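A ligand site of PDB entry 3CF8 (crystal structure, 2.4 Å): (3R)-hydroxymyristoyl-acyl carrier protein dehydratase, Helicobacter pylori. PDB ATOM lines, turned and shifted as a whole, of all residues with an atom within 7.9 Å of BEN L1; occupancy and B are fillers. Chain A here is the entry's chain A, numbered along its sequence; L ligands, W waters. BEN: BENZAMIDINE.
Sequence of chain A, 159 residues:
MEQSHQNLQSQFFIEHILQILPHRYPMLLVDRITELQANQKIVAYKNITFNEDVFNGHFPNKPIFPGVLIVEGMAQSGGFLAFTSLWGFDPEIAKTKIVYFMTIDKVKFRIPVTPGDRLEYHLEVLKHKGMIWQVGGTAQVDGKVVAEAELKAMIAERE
The side-chain amide nitrogen of Gln 40 sits close to a nitrogen (N1) of BEN L1 (3.0 Å).
The side-chain carboxylate of Glu 124 lies within salt-bridge range of a nitrogen (N2) of BEN L1, at 2.7 Å.
The backbone NH of Leu 126 lies within hydrogen-bond range of the backbone carbonyl oxygen of Gln 134, 2.9 Å away.
O of Gln 40 is in hydrogen-bond range of N of Val 125, at 2.8 Å.
The backbone NH (N) of Glu 124 sits at hydrogen-bond distance from the backbone carbonyl oxygen (O) of Gly 136.
Val 125 touches BEN L1 (O to C3, 3.2 Å).
Leu 126 touches BEN L1 (CD2 to C4, 3.96 Å).
Hydrophobic or aromatic side chains within 4 Å of BEN L1: Leu 126.
Along chain A the residues within 4 Å of BEN L1 span positions 40 to 126.
The nearest printed residue that does not touch BEN L1 is Lys 41 (4.1 Å).
Water W1 lies within hydrogen-bond range of NE2 of Gln 40 and N2 of BEN L1.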
ATOM      1  N   GLN A  37      15.855  36.056 -10.005  1.00  0.00           N
ATOM      2  CA  GLN A  37      17.098  35.323 -10.210  1.00  0.00           C
ATOM      3  C   GLN A  37      17.020  34.548 -11.510  1.00  0.00           C
ATOM      4  O   GLN A  37      16.157  33.670 -11.651  1.00  0.00           O
ATOM      5  CB  GLN A  37      17.401  34.387  -9.035  1.00  0.00           C
ATOM      6  CG  GLN A  37      18.117  35.065  -7.861  1.00  0.00           C
ATOM      7  CD  GLN A  37      19.416  35.757  -8.276  1.00  0.00           C
ATOM      8  OE1 GLN A  37      20.346  35.105  -8.796  1.00  0.00           O
ATOM      9  NE2 GLN A  37      19.488  37.072  -8.064  1.00  0.00           N
ATOM     10  N   ALA A  38      17.905  34.872 -12.454  1.00  0.00           N
ATOM     11  CA  ALA A  38      17.937  34.216 -13.760  1.00  0.00           C
ATOM     12  C   ALA A  38      17.899  32.696 -13.638  1.00  0.00           C
ATOM     13  O   ALA A  38      18.612  32.126 -12.806  1.00  0.00           O
ATOM     14  CB  ALA A  38      19.161  34.653 -14.555  1.00  0.00           C
ATOM     15  N   ASN A  39      17.043  32.057 -14.438  1.00  0.00           N
ATOM     16  CA  ASN A  39      16.902  30.586 -14.503  1.00  0.00           C
ATOM     17  C   ASN A  39      16.375  29.921 -13.236  1.00  0.00           C
ATOM     18  O   ASN A  39      16.304  28.695 -13.158  1.00  0.00           O
ATOM     19  CB  ASN A  39      18.233  29.926 -14.892  1.00  0.00           C
ATOM     20  CG  ASN A  39      18.823  30.513 -16.148  1.00  0.00           C
ATOM     21  OD1 ASN A  39      19.844  31.188 -16.097  1.00  0.00           O
ATOM     22  ND2 ASN A  39      18.184  30.259 -17.280  1.00  0.00           N
ATOM     23  N   GLN A  40      15.994  30.723 -12.247  1.00  0.00           N
ATOM     24  CA  GLN A  40      15.610  30.178 -10.949  1.00  0.00           C
ATOM     25  C   GLN A  40      14.239  30.648 -10.486  1.00  0.00           C
ATOM     26  O   GLN A  40      13.341  29.825 -10.252  1.00  0.00           O
ATOM     27  CB  GLN A  40      16.656  30.504  -9.895  1.00  0.00           C
ATOM     28  CG  GLN A  40      17.951  29.726 -10.059  1.00  0.00           C
ATOM     29  CD  GLN A  40      18.819  29.799  -8.828  1.00  0.00           C
ATOM     30  OE1 GLN A  40      19.992  30.174  -8.908  1.00  0.00           O
ATOM     31  NE2 GLN A  40      18.247  29.470  -7.679  1.00  0.00           N
ATOM     32  N   LYS A  41      14.084  31.952 -10.313  1.00  0.00           N
ATOM     33  CA  LYS A  41      12.838  32.477  -9.770  1.00  0.00           C
ATOM     34  C   LYS A  41      12.538  33.957 -10.001  1.00  0.00           C
ATOM     35  O   LYS A  41      13.414  34.748 -10.359  1.00  0.00           O
ATOM     36  CB  LYS A  41      12.708  32.132  -8.280  1.00  0.00           C
ATOM     37  CG  LYS A  41      13.415  33.033  -7.314  1.00  0.00           C
ATOM     38  CD  LYS A  41      12.726  32.887  -5.974  1.00  0.00           C
ATOM     39  CE  LYS A  41      13.332  33.787  -4.923  1.00  0.00           C
ATOM     40  NZ  LYS A  41      12.479  33.810  -3.676  1.00  0.00           N
ATOM     41  N   ILE A  42      11.267  34.292  -9.791  1.00  0.00           N
ATOM     42  CA  ILE A  42      10.754  35.649  -9.871  1.00  0.00           C
ATOM     43  C   ILE A  42       9.689  35.830  -8.788  1.00  0.00           C
ATOM     44  O   ILE A  42       8.888  34.937  -8.518  1.00  0.00           O
ATOM     45  CB  ILE A  42      10.172  35.970 -11.296  1.00  0.00           C
ATOM     46  CG1 ILE A  42       9.813  37.459 -11.422  1.00  0.00           C
ATOM     47  CG2 ILE A  42       9.002  35.040 -11.655  1.00  0.00           C
ATOM     48  CD1 ILE A  42       9.391  37.904 -12.813  1.00  0.00           C
ATOM     49  N   LEU A 123       6.976  32.543  -8.610  1.00  0.00           N
ATOM     50  CA  LEU A 123       7.227  31.492  -9.596  1.00  0.00           C
ATOM     51  C   LEU A 123       8.666  31.014  -9.532  1.00  0.00           C
ATOM     52  O   LEU A 123       9.589  31.803  -9.310  1.00  0.00           O
ATOM     53  CB  LEU A 123       6.914  31.977 -11.022  1.00  0.00           C
ATOM     54  CG  LEU A 123       5.463  32.103 -11.518  1.00  0.00           C
ATOM     55  CD1 LEU A 123       4.740  30.747 -11.545  1.00  0.00           C
ATOM     56  CD2 LEU A 123       4.678  33.141 -10.696  1.00  0.00           C
ATOM     57  N   GLU A 124       8.834  29.714  -9.736  1.00  0.00           N
ATOM     58  CA  GLU A 124      10.154  29.115  -9.752  1.00  0.00           C
ATOM     59  C   GLU A 124      10.307  28.159 -10.919  1.00  0.00           C
ATOM     60  O   GLU A 124       9.324  27.534 -11.351  1.00  0.00           O
ATOM     61  CB  GLU A 124      10.460  28.483  -8.382  1.00  0.00           C
ATOM     62  CG  GLU A 124      10.517  29.582  -7.302  1.00  0.00           C
ATOM     63  CD  GLU A 124      10.786  29.086  -5.911  1.00  0.00           C
ATOM     64  OE1 GLU A 124      10.023  28.242  -5.402  1.00  0.00           O
ATOM     65  OE2 GLU A 124      11.769  29.582  -5.310  1.00  0.00           O
ATOM     66  N   VAL A 125      11.515  28.086 -11.460  1.00  0.00           N
ATOM     67  CA  VAL A 125      11.800  27.277 -12.647  1.00  0.00           C
ATOM     68  C   VAL A 125      12.010  25.799 -12.285  1.00  0.00           C
ATOM     69  O   VAL A 125      12.957  25.444 -11.566  1.00  0.00           O
ATOM     70  CB  VAL A 125      13.020  27.816 -13.442  1.00  0.00           C
ATOM     71  CG1 VAL A 125      13.246  27.023 -14.734  1.00  0.00           C
ATOM     72  CG2 VAL A 125      12.837  29.293 -13.743  1.00  0.00           C
ATOM     73  N   LEU A 126      11.099  24.952 -12.759  1.00  0.00           N
ATOM     74  CA  LEU A 126      11.170  23.519 -12.504  1.00  0.00           C
ATOM     75  C   LEU A 126      12.024  22.815 -13.550  1.00  0.00           C
ATOM     76  O   LEU A 126      12.784  21.897 -13.237  1.00  0.00           O
ATOM     77  CB  LEU A 126       9.761  22.916 -12.438  1.00  0.00           C
ATOM     78  CG  LEU A 126       8.746  23.577 -11.491  1.00  0.00           C
ATOM     79  CD1 LEU A 126       7.416  22.845 -11.548  1.00  0.00           C
ATOM     80  CD2 LEU A 126       9.267  23.643 -10.049  1.00  0.00           C
ATOM     81  N   LYS A 127      11.917  23.287 -14.801  1.00  0.00           N
ATOM     82  CA  LYS A 127      12.731  22.794 -15.913  1.00  0.00           C
ATOM     83  C   LYS A 127      12.797  23.811 -17.051  1.00  0.00           C
ATOM     84  O   LYS A 127      11.797  24.457 -17.383  1.00  0.00           O
ATOM     85  CB  LYS A 127      12.190  21.465 -16.429  1.00  0.00           C
ATOM     86  CG  LYS A 127      13.051  20.830 -17.505  1.00  0.00           C
ATOM     87  CD  LYS A 127      12.471  19.512 -18.000  1.00  0.00           C
ATOM     88  CE  LYS A 127      13.240  19.031 -19.218  1.00  0.00           C
ATOM     89  NZ  LYS A 127      12.818  17.643 -19.578  1.00  0.00           N
ATOM     90  N   GLN A 134       9.278  25.447 -18.002  1.00  0.00           N
ATOM     91  CA  GLN A 134       8.312  24.830 -17.106  1.00  0.00           C
ATOM     92  C   GLN A 134       8.476  25.481 -15.739  1.00  0.00           C
ATOM     93  O   GLN A 134       9.533  25.365 -15.108  1.00  0.00           O
ATOM     94  CB  GLN A 134       8.589  23.327 -17.029  1.00  0.00           C
ATOM     95  CG  GLN A 134       7.455  22.488 -16.498  1.00  0.00           C
ATOM     96  CD  GLN A 134       7.472  21.051 -17.033  1.00  0.00           C
ATOM     97  OE1 GLN A 134       6.703  20.207 -16.575  1.00  0.00           O
ATOM     98  NE2 GLN A 134       8.356  20.780 -18.008  1.00  0.00           N
ATOM     99  N   GLY A 136       6.499  26.782 -11.835  1.00  0.00           N
ATOM    100  CA  GLY A 136       5.483  26.450 -10.854  1.00  0.00           C
ATOM    101  C   GLY A 136       5.627  27.386  -9.672  1.00  0.00           C
ATOM    102  O   GLY A 136       6.704  27.948  -9.447  1.00  0.00           O
HETATM  103  C1  BEN L   1      13.648  26.807  -7.199  1.00  0.00           C
HETATM  104  C2  BEN L   1      13.641  26.018  -8.350  1.00  0.00           C
HETATM  105  C3  BEN L   1      12.828  24.881  -8.432  1.00  0.00           C
HETATM  106  C4  BEN L   1      12.029  24.527  -7.357  1.00  0.00           C
HETATM  107  C5  BEN L   1      12.020  25.303  -6.199  1.00  0.00           C
HETATM  108  C6  BEN L   1      12.832  26.441  -6.117  1.00  0.00           C
HETATM  109  C   BEN L   1      14.475  27.941  -7.118  1.00  0.00           C
HETATM  110  N1  BEN L   1      15.561  28.052  -7.868  1.00  0.00           N
HETATM  111  N2  BEN L   1      14.232  28.947  -6.290  1.00  0.00           N
HETATM  112  C1  BEN L   2       3.918  25.241  -4.190  1.00  0.00           C
HETATM  113  C2  BEN L   2       2.870  24.390  -4.556  1.00  0.00           C
HETATM  114  C3  BEN L   2       1.867  24.078  -3.646  1.00  0.00           C
HETATM  115  C4  BEN L   2       1.886  24.624  -2.350  1.00  0.00           C
HETATM  116  C5  BEN L   2       2.920  25.470  -1.971  1.00  0.00           C
HETATM  117  C6  BEN L   2       3.928  25.776  -2.893  1.00  0.00           C
HETATM  118  C   BEN L   2       4.945  25.559  -5.102  1.00  0.00           C
HETATM  119  N1  BEN L   2       5.087  24.923  -6.252  1.00  0.00           N
HETATM  120  N2  BEN L   2       5.839  26.509  -4.842  1.00  0.00           N
HETATM  121  O   HOH W   1      16.494  31.400  -6.433  1.00  0.00           O
